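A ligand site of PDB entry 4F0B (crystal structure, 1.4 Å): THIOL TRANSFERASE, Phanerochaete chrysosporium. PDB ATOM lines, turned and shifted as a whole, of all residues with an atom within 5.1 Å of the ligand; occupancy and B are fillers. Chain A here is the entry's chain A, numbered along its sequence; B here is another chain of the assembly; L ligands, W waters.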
ATOM      1  N   THR A  16     -26.566  -0.470  26.018  1.00  0.00           N
ATOM      2  CA  THR A  16     -26.443   0.929  26.457  1.00  0.00           C
ATOM      3  C   THR A  16     -26.534   1.821  25.217  1.00  0.00           C
ATOM      4  O   THR A  16     -26.385   1.349  24.080  1.00  0.00           O
ATOM      5  CB  THR A  16     -25.060   1.223  27.096  1.00  0.00           C
ATOM      6  OG1 THR A  16     -24.046   0.909  26.129  1.00  0.00           O
ATOM      7  CG2 THR A  16     -24.764   0.344  28.302  1.00  0.00           C
ATOM      8  N   PRO A  17     -26.744   3.131  25.395  1.00  0.00           N
ATOM      9  CA  PRO A  17     -26.849   4.040  24.239  1.00  0.00           C
ATOM     10  C   PRO A  17     -25.631   4.054  23.329  1.00  0.00           C
ATOM     11  O   PRO A  17     -25.754   4.353  22.125  1.00  0.00           O
ATOM     12  CB  PRO A  17     -27.056   5.445  24.900  1.00  0.00           C
ATOM     13  CG  PRO A  17     -26.596   5.246  26.345  1.00  0.00           C
ATOM     14  CD  PRO A  17     -26.995   3.836  26.681  1.00  0.00           C
ATOM     15  N   ASN A  18     -24.445   3.735  23.871  1.00  0.00           N
ATOM     16  CA  ASN A  18     -23.272   3.566  23.039  1.00  0.00           C
ATOM     17  C   ASN A  18     -23.113   2.139  22.494  1.00  0.00           C
ATOM     18  O   ASN A  18     -22.771   1.948  21.313  1.00  0.00           O
ATOM     19  CB  ASN A  18     -22.006   3.979  23.831  1.00  0.00           C
ATOM     20  CG  ASN A  18     -21.980   5.483  24.080  1.00  0.00           C
ATOM     21  OD1 ASN A  18     -22.315   6.265  23.181  1.00  0.00           O
ATOM     22  ND2 ASN A  18     -21.611   5.880  25.288  1.00  0.00           N
ATOM     23  N   GLY A  19     -23.338   1.145  23.347  1.00  0.00           N
ATOM     24  CA  GLY A  19     -23.202  -0.254  22.936  1.00  0.00           C
ATOM     25  C   GLY A  19     -24.091  -0.689  21.790  1.00  0.00           C
ATOM     26  O   GLY A  19     -23.691  -1.534  20.978  1.00  0.00           O
ATOM     27  N   ILE A  45     -19.862  -3.452  32.553  1.00  0.00           N
ATOM     28  CA  ILE A  45     -19.416  -2.057  32.647  1.00  0.00           C
ATOM     29  C   ILE A  45     -19.526  -1.572  34.082  1.00  0.00           C
ATOM     30  O   ILE A  45     -19.460  -0.366  34.329  1.00  0.00           O
ATOM     31  CB  ILE A  45     -20.246  -1.115  31.723  1.00  0.00           C
ATOM     32  CG1 ILE A  45     -21.708  -1.161  32.131  1.00  0.00           C
ATOM     33  CG2 ILE A  45     -20.031  -1.537  30.282  1.00  0.00           C
ATOM     34  CD1 ILE A  45     -22.560  -0.045  31.503  1.00  0.00           C
ATOM     35  N   ASP A  47     -18.274  -1.007  37.903  1.00  0.00           N
ATOM     36  CA  ASP A  47     -17.109  -0.956  38.777  1.00  0.00           C
ATOM     37  C   ASP A  47     -17.108  -2.076  39.845  1.00  0.00           C
ATOM     38  O   ASP A  47     -16.047  -2.541  40.235  1.00  0.00           O
ATOM     39  CB  ASP A  47     -17.008   0.427  39.460  1.00  0.00           C
ATOM     40  CG  ASP A  47     -16.708   1.562  38.489  1.00  0.00           C
ATOM     41  OD1 ASP A  47     -16.298   1.294  37.341  1.00  0.00           O
ATOM     42  OD2 ASP A  47     -16.862   2.749  38.882  1.00  0.00           O
ATOM     43  N   VAL A  57     -14.771  -4.318  31.579  1.00  0.00           N
ATOM     44  CA  VAL A  57     -14.072  -3.325  30.766  1.00  0.00           C
ATOM     45  C   VAL A  57     -12.727  -2.852  31.241  1.00  0.00           C
ATOM     46  O   VAL A  57     -11.970  -2.326  30.430  1.00  0.00           O
ATOM     47  CB  VAL A  57     -14.946  -2.078  30.477  1.00  0.00           C
ATOM     48  CG1 VAL A  57     -16.163  -2.484  29.609  1.00  0.00           C
ATOM     49  CG2 VAL A  57     -15.375  -1.410  31.770  1.00  0.00           C
ATOM     50  N   LYS A  58     -12.389  -3.076  32.526  1.00  0.00           N
ATOM     51  CA  LYS A  58     -11.078  -2.656  33.037  1.00  0.00           C
ATOM     52  C   LYS A  58     -10.057  -3.794  33.053  1.00  0.00           C
ATOM     53  O   LYS A  58      -8.915  -3.600  33.498  1.00  0.00           O
ATOM     54  CB  LYS A  58     -11.215  -2.064  34.438  1.00  0.00           C
ATOM     55  CG  LYS A  58     -12.183  -0.854  34.535  1.00  0.00           C
ATOM     56  CD  LYS A  58     -11.881   0.174  33.425  1.00  0.00           C
ATOM     57  CE  LYS A  58     -12.809   1.407  33.566  1.00  0.00           C
ATOM     58  NZ  LYS A  58     -12.595   2.359  32.433  1.00  0.00           N
ATOM     59  N   GLY A  69     -10.736   1.412  28.269  1.00  0.00           N
ATOM     60  CA  GLY A  69     -11.486   0.554  29.182  1.00  0.00           C
ATOM     61  C   GLY A  69     -12.981   0.815  29.208  1.00  0.00           C
ATOM     62  O   GLY A  69     -13.584   0.901  30.271  1.00  0.00           O
ATOM     63  N   ARG A  70     -13.582   0.951  28.016  1.00  0.00           N
ATOM     64  CA  ARG A  70     -15.026   1.191  27.894  1.00  0.00           C
ATOM     65  C   ARG A  70     -15.526   0.453  26.658  1.00  0.00           C
ATOM     66  O   ARG A  70     -14.743   0.127  25.750  1.00  0.00           O
ATOM     67  CB  ARG A  70     -15.336   2.684  27.717  1.00  0.00           C
ATOM     68  CG  ARG A  70     -15.088   3.504  28.987  1.00  0.00           C
ATOM     69  CD  ARG A  70     -15.981   4.773  28.995  1.00  0.00           C
ATOM     70  NE  ARG A  70     -15.705   5.587  30.140  1.00  0.00           N
ATOM     71  CZ  ARG A  70     -16.286   6.750  30.350  1.00  0.00           C
ATOM     72  NH1 ARG A  70     -17.176   7.195  29.485  1.00  0.00           N
ATOM     73  NH2 ARG A  70     -15.931   7.461  31.435  1.00  0.00           N
ATOM     74  N   ILE A  71     -16.826   0.124  26.651  1.00  0.00           N
ATOM     75  CA  ILE A  71     -17.446  -0.404  25.428  1.00  0.00           C
ATOM     76  C   ILE A  71     -18.133   0.748  24.665  1.00  0.00           C
ATOM     77  O   ILE A  71     -18.430   1.805  25.216  1.00  0.00           O
ATOM     78  CB  ILE A  71     -18.446  -1.563  25.714  1.00  0.00           C
ATOM     79  CG1 ILE A  71     -19.581  -1.176  26.656  1.00  0.00           C
ATOM     80  CG2 ILE A  71     -17.723  -2.792  26.249  1.00  0.00           C
ATOM     81  CD1 ILE A  71     -20.747  -0.436  25.969  1.00  0.00           C
ATOM     82  N   PRO A  72     -18.394   0.552  23.374  1.00  0.00           N
ATOM     83  CA  PRO A  72     -18.061  -0.630  22.568  1.00  0.00           C
ATOM     84  C   PRO A  72     -16.678  -0.542  21.969  1.00  0.00           C
ATOM     85  O   PRO A  72     -16.021   0.508  21.910  1.00  0.00           O
ATOM     86  CB  PRO A  72     -19.124  -0.582  21.451  1.00  0.00           C
ATOM     87  CG  PRO A  72     -19.327   0.938  21.239  1.00  0.00           C
ATOM     88  CD  PRO A  72     -19.218   1.549  22.637  1.00  0.00           C
ATOM     89  N   GLU A  83     -14.201   3.604  20.358  1.00  0.00           N
ATOM     90  CA  GLU A  83     -15.040   4.830  20.217  1.00  0.00           C
ATOM     91  C   GLU A  83     -16.167   4.603  19.213  1.00  0.00           C
ATOM     92  O   GLU A  83     -15.919   4.402  18.012  1.00  0.00           O
ATOM     93  CB  GLU A  83     -14.219   6.069  19.822  1.00  0.00           C
ATOM     94  CG  GLU A  83     -13.188   6.480  20.873  1.00  0.00           C
ATOM     95  CD  GLU A  83     -13.796   7.068  22.133  1.00  0.00           C
ATOM     96  OE1 GLU A  83     -14.855   7.745  22.028  1.00  0.00           O
ATOM     97  OE2 GLU A  83     -13.268   6.831  23.232  1.00  0.00           O
ATOM     98  N   THR A  84     -17.405   4.629  19.722  1.00  0.00           N
ATOM     99  CA  THR A  84     -18.606   4.416  18.888  1.00  0.00           C
ATOM    100  C   THR A  84     -18.475   4.978  17.470  1.00  0.00           C
ATOM    101  O   THR A  84     -18.587   4.213  16.499  1.00  0.00           O
ATOM    102  CB  THR A  84     -19.867   5.094  19.526  1.00  0.00           C
ATOM    103  OG1 THR A  84     -19.548   6.446  19.871  1.00  0.00           O
ATOM    104  CG2 THR A  84     -20.335   4.313  20.735  1.00  0.00           C
ATOM    105  N   SER A  85     -18.276   6.292  17.347  1.00  0.00           N
ATOM    106  CA  SER A  85     -18.327   6.939  16.034  1.00  0.00           C
ATOM    107  C   SER A  85     -17.221   6.467  15.123  1.00  0.00           C
ATOM    108  O   SER A  85     -17.451   6.293  13.899  1.00  0.00           O
ATOM    109  CB  SER A  85     -18.251   8.445  16.221  1.00  0.00           C
ATOM    110  OG  SER A  85     -19.352   8.849  17.045  1.00  0.00           O
ATOM    111  N   HIS A 123     -20.793  13.168  19.409  1.00  0.00           N
ATOM    112  CA  HIS A 123     -19.773  12.515  20.209  1.00  0.00           C
ATOM    113  C   HIS A 123     -19.236  13.450  21.320  1.00  0.00           C
ATOM    114  O   HIS A 123     -18.808  12.983  22.384  1.00  0.00           O
ATOM    115  CB  HIS A 123     -18.654  12.090  19.284  1.00  0.00           C
ATOM    116  CG  HIS A 123     -17.857  10.962  19.798  1.00  0.00           C
ATOM    117  ND1 HIS A 123     -18.143   9.633  19.490  1.00  0.00           N
ATOM    118  CD2 HIS A 123     -16.750  10.949  20.591  1.00  0.00           C
ATOM    119  CE1 HIS A 123     -17.249   8.863  20.095  1.00  0.00           C
ATOM    120  NE2 HIS A 123     -16.382   9.633  20.748  1.00  0.00           N
ATOM    121  N   GLY A 127     -23.804  12.708  23.526  1.00  0.00           N
ATOM    122  CA  GLY A 127     -23.409  11.580  24.335  1.00  0.00           C
ATOM    123  C   GLY A 127     -22.835  12.009  25.691  1.00  0.00           C
ATOM    124  O   GLY A 127     -23.299  11.557  26.759  1.00  0.00           O
ATOM    125  N   PRO A 128     -21.856  12.919  25.699  1.00  0.00           N
ATOM    126  CA  PRO A 128     -21.277  13.329  26.994  1.00  0.00           C
ATOM    127  C   PRO A 128     -22.330  14.012  27.876  1.00  0.00           C
ATOM    128  O   PRO A 128     -22.418  13.700  29.076  1.00  0.00           O
ATOM    129  CB  PRO A 128     -20.188  14.320  26.585  1.00  0.00           C
ATOM    130  CG  PRO A 128     -19.704  13.753  25.220  1.00  0.00           C
ATOM    131  CD  PRO A 128     -20.991  13.288  24.562  1.00  0.00           C
ATOM    132  N   GLY A 131     -25.192  11.800  28.923  1.00  0.00           N
ATOM    133  CA  GLY A 131     -24.611  10.830  29.839  1.00  0.00           C
ATOM    134  C   GLY A 131     -24.461  11.435  31.240  1.00  0.00           C
ATOM    135  O   GLY A 131     -24.653  10.734  32.246  1.00  0.00           O
ATOM    136  N   GLN A 132     -24.148  12.731  31.314  1.00  0.00           N
ATOM    137  CA  GLN A 132     -24.032  13.378  32.634  1.00  0.00           C
ATOM    138  C   GLN A 132     -25.410  13.555  33.219  1.00  0.00           C
ATOM    139  O   GLN A 132     -25.587  13.420  34.432  1.00  0.00           O
ATOM    140  CB  GLN A 132     -23.316  14.734  32.550  1.00  0.00           C
ATOM    141  CG  GLN A 132     -21.867  14.674  31.988  1.00  0.00           C
ATOM    142  CD  GLN A 132     -21.122  13.409  32.349  1.00  0.00           C
ATOM    143  OE1 GLN A 132     -20.746  13.193  33.513  1.00  0.00           O
ATOM    144  NE2 GLN A 132     -20.926  12.556  31.360  1.00  0.00           N
ATOM    145  N   HIS A 135     -26.244  10.375  34.637  1.00  0.00           N
ATOM    146  CA  HIS A 135     -25.512  10.134  35.886  1.00  0.00           C
ATOM    147  C   HIS A 135     -26.188  10.828  37.071  1.00  0.00           C
ATOM    148  O   HIS A 135     -26.528  10.206  38.065  1.00  0.00           O
ATOM    149  CB  HIS A 135     -24.063  10.599  35.813  1.00  0.00           C
ATOM    150  CG  HIS A 135     -23.339  10.320  37.086  1.00  0.00           C
ATOM    151  ND1 HIS A 135     -22.981   9.026  37.434  1.00  0.00           N
ATOM    152  CD2 HIS A 135     -23.024  11.097  38.138  1.00  0.00           C
ATOM    153  CE1 HIS A 135     -22.432   9.051  38.631  1.00  0.00           C
ATOM    154  NE2 HIS A 135     -22.450  10.287  39.085  1.00  0.00           N
ATOM    155  N   LYS A 182     -25.705   6.866  15.259  1.00  0.00           N
ATOM    156  CA  LYS A 182     -24.969   7.310  16.442  1.00  0.00           C
ATOM    157  C   LYS A 182     -25.857   8.032  17.440  1.00  0.00           C
ATOM    158  O   LYS A 182     -25.853   7.723  18.649  1.00  0.00           O
ATOM    159  CB  LYS A 182     -23.800   8.217  16.041  1.00  0.00           C
ATOM    160  CG  LYS A 182     -23.152   8.941  17.245  1.00  0.00           C
ATOM    161  CD  LYS A 182     -22.483   8.002  18.242  1.00  0.00           C
ATOM    162  CE  LYS A 182     -22.163   8.772  19.542  1.00  0.00           C
ATOM    163  NZ  LYS A 182     -21.819   7.834  20.662  1.00  0.00           N
ATOM    164  N   TRP A 186     -28.731   7.297  21.837  1.00  0.00           N
ATOM    165  CA  TRP A 186     -29.047   8.216  22.928  1.00  0.00           C
ATOM    166  C   TRP A 186     -30.479   8.740  22.898  1.00  0.00           C
ATOM    167  O   TRP A 186     -31.158   8.831  23.922  1.00  0.00           O
ATOM    168  CB  TRP A 186     -28.028   9.358  22.960  1.00  0.00           C
ATOM    169  CG  TRP A 186     -26.707   8.938  23.500  1.00  0.00           C
ATOM    170  CD1 TRP A 186     -25.602   8.538  22.783  1.00  0.00           C
ATOM    171  CD2 TRP A 186     -26.366   8.854  24.876  1.00  0.00           C
ATOM    172  NE1 TRP A 186     -24.576   8.189  23.651  1.00  0.00           N
ATOM    173  CE2 TRP A 186     -25.026   8.375  24.952  1.00  0.00           C
ATOM    174  CE3 TRP A 186     -27.078   9.119  26.067  1.00  0.00           C
ATOM    175  CZ2 TRP A 186     -24.358   8.202  26.164  1.00  0.00           C
ATOM    176  CZ3 TRP A 186     -26.418   8.927  27.287  1.00  0.00           C
ATOM    177  CH2 TRP A 186     -25.062   8.474  27.319  1.00  0.00           C
ATOM    178  N   PHE B 120     -11.676  10.892  18.265  1.00  0.00           N
ATOM    179  CA  PHE B 120     -12.940  10.665  18.961  1.00  0.00           C
ATOM    180  C   PHE B 120     -12.731  10.448  20.456  1.00  0.00           C
ATOM    181  O   PHE B 120     -13.559  10.906  21.251  1.00  0.00           O
ATOM    182  CB  PHE B 120     -13.758   9.545  18.271  1.00  0.00           C
ATOM    183  CG  PHE B 120     -14.502   9.991  17.054  1.00  0.00           C
ATOM    184  CD1 PHE B 120     -15.672  10.762  17.167  1.00  0.00           C
ATOM    185  CD2 PHE B 120     -14.091   9.603  15.771  1.00  0.00           C
ATOM    186  CE1 PHE B 120     -16.384  11.147  16.046  1.00  0.00           C
ATOM    187  CE2 PHE B 120     -14.814   9.997  14.647  1.00  0.00           C
ATOM    188  CZ  PHE B 120     -15.974  10.772  14.790  1.00  0.00           C
ATOM    189  N   GLY B 124     -14.755  12.955  22.873  1.00  0.00           N
ATOM    190  CA  GLY B 124     -15.750  12.460  23.804  1.00  0.00           C
ATOM    191  C   GLY B 124     -15.290  12.333  25.246  1.00  0.00           C
ATOM    192  O   GLY B 124     -16.133  12.130  26.117  1.00  0.00           O
ATOM    193  N   ARG B 150     -15.680  14.068  40.954  1.00  0.00           N
ATOM    194  CA  ARG B 150     -16.031  13.253  39.784  1.00  0.00           C
ATOM    195  C   ARG B 150     -15.212  13.640  38.552  1.00  0.00           C
ATOM    196  O   ARG B 150     -14.621  12.791  37.876  1.00  0.00           O
ATOM    197  CB  ARG B 150     -17.539  13.369  39.492  1.00  0.00           C
ATOM    198  CG  ARG B 150     -17.946  12.701  38.161  1.00  0.00           C
ATOM    199  CD  ARG B 150     -19.486  12.731  38.043  1.00  0.00           C
ATOM    200  NE  ARG B 150     -19.929  12.315  36.713  1.00  0.00           N
ATOM    201  CZ  ARG B 150     -20.021  11.055  36.311  1.00  0.00           C
ATOM    202  NH1 ARG B 150     -19.672  10.041  37.106  1.00  0.00           N
ATOM    203  NH2 ARG B 150     -20.424  10.783  35.077  1.00  0.00           N
HETATM  204  N1  LIG L   1     -16.798   8.037  23.903  1.00  0.00           N
HETATM  205  C1  LIG L   1     -17.031   6.569  24.106  1.00  0.00           C
HETATM  206  C2  LIG L   1     -17.717   6.025  22.821  1.00  0.00           C
HETATM  207  O1  LIG L   1     -18.413   6.801  22.135  1.00  0.00           O
HETATM  208  O2  LIG L   1     -17.520   4.823  22.541  1.00  0.00           O
HETATM  209  C3  LIG L   1     -17.982   6.376  25.293  1.00  0.00           C
HETATM  210  C4  LIG L   1     -18.177   4.882  25.628  1.00  0.00           C
HETATM  211  C5  LIG L   1     -18.848   4.757  26.986  1.00  0.00           C
HETATM  212  O3  LIG L   1     -19.212   5.685  27.691  1.00  0.00           O
HETATM  213  N2  LIG L   1     -18.960   3.462  27.444  1.00  0.00           N
HETATM  214  C6  LIG L   1     -19.597   3.122  28.733  1.00  0.00           C
HETATM  215  C7  LIG L   1     -18.669   2.234  29.519  1.00  0.00           C
HETATM  216  O4  LIG L   1     -18.036   1.292  28.972  1.00  0.00           O
HETATM  217  C8  LIG L   1     -20.918   2.381  28.565  1.00  0.00           C
HETATM  218  S1  LIG L   1     -22.132   3.212  27.544  1.00  0.00           S
HETATM  219  N3  LIG L   1     -18.614   2.512  30.840  1.00  0.00           N
HETATM  220  C9  LIG L   1     -17.781   1.684  31.716  1.00  0.00           C
HETATM  221  C10 LIG L   1     -16.877   2.488  32.584  1.00  0.00           C
HETATM  222  O5  LIG L   1     -16.107   1.842  33.321  1.00  0.00           O
HETATM  223  O6  LIG L   1     -16.912   3.746  32.510  1.00  0.00           O
HETATM  224  N4  LIG L   1     -20.935   7.949  28.212  1.00  0.00           N
HETATM  225  C11 LIG L   1     -20.636   9.302  27.794  1.00  0.00           C
HETATM  226  C12 LIG L   1     -20.404   9.464  26.261  1.00  0.00           C
HETATM  227  O7  LIG L   1     -20.883   8.622  25.470  1.00  0.00           O
HETATM  228  O8  LIG L   1     -19.727  10.452  25.919  1.00  0.00           O
HETATM  229  C13 LIG L   1     -21.750   7.737  29.253  1.00  0.00           C
HETATM  230  O9  LIG L   1     -22.276   8.678  29.891  1.00  0.00           O
HETATM  231  C14 LIG L   1     -21.994   6.291  29.647  1.00  0.00           C
HETATM  232  N5  LIG L   1     -22.058   6.180  31.126  1.00  0.00           N
HETATM  233  C15 LIG L   1     -23.316   5.877  28.966  1.00  0.00           C
HETATM  234  S2  LIG L   1     -23.601   4.120  29.132  1.00  0.00           S
HETATM  235  C16 LIG L   1     -18.903   6.115  33.932  1.00  0.00           C
HETATM  236  C17 LIG L   1     -19.235   7.481  34.550  1.00  0.00           C
HETATM  237  O10 LIG L   1     -19.589   8.408  33.790  1.00  0.00           O
HETATM  238  O11 LIG L   1     -19.072   7.591  35.800  1.00  0.00           O
HETATM  239  N6  LIG L   1     -17.724   5.589  34.601  1.00  0.00           N
HETATM  240  C18 LIG L   1     -20.102   5.126  34.100  1.00  0.00           C
HETATM  241  C19 LIG L   1     -21.408   5.464  33.323  1.00  0.00           C
HETATM  242  C20 LIG L   1     -21.183   5.412  31.847  1.00  0.00           C
HETATM  243  O12 LIG L   1     -20.294   4.783  31.278  1.00  0.00           O
HETATM  244  O   HOH W   1     -14.345   4.621  32.645  1.00  0.00           O
HETATM  245  O   HOH W   2     -21.116   9.362  22.849  1.00  0.00           O
HETATM  246  O   HOH W   3     -24.166   7.800  32.645  1.00  0.00           O
HETATM  247  O   HOH W   4     -17.891   4.827  37.319  1.00  0.00           O
HETATM  248  O   HOH W   5     -15.497   3.142  35.648  1.00  0.00           O
HETATM  249  O   HOH W   6     -18.297  11.865  27.820  1.00  0.00           O
HETATM  250  O   HOH W   7     -18.579  10.368  23.431  1.00  0.00           O
HETATM  251  O   HOH W   8     -17.029   9.898  32.795  1.00  0.00           O
HETATM  252  O   HOH W   9     -15.467   2.998  23.025  1.00  0.00           O
HETATM  253  O   HOH W  10     -18.749   2.154  35.346  1.00  0.00           O
HETATM  254  O   HOH W  11     -20.195   9.733  31.502  1.00  0.00           O
HETATM  255  O   HOH W  12     -20.500   6.115  38.150  1.00  0.00           O
HETATM  256  O   HOH W  13     -14.876   6.516  34.433  1.00  0.00           O
HETATM  257  O   HOH W  14     -16.836   9.277  26.460  1.00  0.00           O
HETATM  258  O   HOH W  15     -15.960  -0.525  35.097  1.00  0.00           O
HETATM  259  O   HOH W  16     -16.559   9.532  35.480  1.00  0.00           O
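Water W11 bridges O10 of the ligand (2.7 Å) and NE2 of Gln 132 (2.9 Å). Water W2 lies within hydrogen-bond range of an oxygen (O7) of the ligand, the side-chain amino group (NZ) of Lys 182 and the side-chain amide oxygen (OD1) of Asn 18. Water W5 lies within hydrogen-bond range of OD1 of Asp 47 and O5 of the ligand. Water W6 lies within hydrogen-bond range of O of Gly 124 of chain B (2.8 Å) and O8 of the ligand (2.8 Å). Water W8 bridges NH2 of Arg 70 (3.0 Å) and O10 of the ligand (3.1 Å). Water W10 lies within hydrogen-bond range of O of Ile 45 (2.8 Å), OD1 of Asp 47 (3.3 Å) and O5 of the ligand (3.3 Å).
A nitrogen (N2) of the ligand sits at hydrogen-bond distance from the backbone carbonyl oxygen of Ile 71, at 2.8 Å. The side-chain amino group (NZ) of Lys 182 is in salt-bridge range of an oxygen (O1) of the ligand, 3.9 Å away. O2 of the ligand lies within hydrogen-bond range of N of Thr 84, at 2.8 Å. OG1 of Thr 84 is in hydrogen-bond range of O1 of the ligand, at 2.6 Å. The side-chain amide nitrogen (ND2) of Asn 18 lies within hydrogen-bond range of an oxygen (O7) of the ligand (2.8 Å). NZ of Lys 58 lies within salt-bridge range of O5 of the ligand (3.7 Å). The side-chain carboxylate (OE1) of Glu 83 lies within salt-bridge range of a nitrogen (N1) of the ligand, 2.7 Å away. N of Ile 71 is in hydrogen-bond range of O4 of the ligand (2.9 Å). The guanidinium group (NE) of Arg 70 is in salt-bridge range of an oxygen (O6) of the ligand, at 3.2 Å. An oxygen (O10) of the ligand is in salt-bridge range of the guanidinium group (NH2) of Arg 150 of chain B (2.8 Å). OG1 of Thr 16 sits close to S1 of the ligand, 3.3 Å away.
NE1 of Trp 186 lies within hydrogen-bond range of OD1 of Asn 18. N of Gly 19 sits at hydrogen-bond distance from OG1 of Thr 16, at 2.9 Å. OE1 of Glu 83 is in hydrogen-bond range of NE2 of His 123 (2.7 Å). The guanidinium group (NH1) of Arg 150 of chain B sits close to a ring nitrogen (NE2) of His 135 (3.4 Å). NZ of Lys 58 is in hydrogen-bond range of O of Gly 69, at 2.8 Å. OD1 of Asn 18 lies within hydrogen-bond range of NZ of Lys 182 (3.0 Å). NE2 of Gln 132 is in hydrogen-bond range of O of Pro 128, at 3.0 Å. The guanidinium group of Arg 150 of chain B lies within hydrogen-bond range of the side-chain amide oxygen of Gln 132 (2.9 Å).
An oxygen (O8) of the ligand sits close to the backbone nitrogen of Pro 128. CG2 of Ile 45 touches O4 of the ligand, 3.7 Å away. CG2 of Val 57 touches O5 of the ligand, 3.7 Å away. Pro 72 touches the ligand. CE1 of His 123 touches O1 of the ligand, 3.1 Å away. Gly 127 touches the ligand (C to O8, 3.5 Å). Gly 131 touches the ligand. Trp 186 touches the ligand (CH2 to C15, 3.5 Å). O of Gly 124 of chain B touches O8 of the ligand, 3.97 Å away. The nearest printed residue that does not touch the ligand is Asp 47 (4.1 Å).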
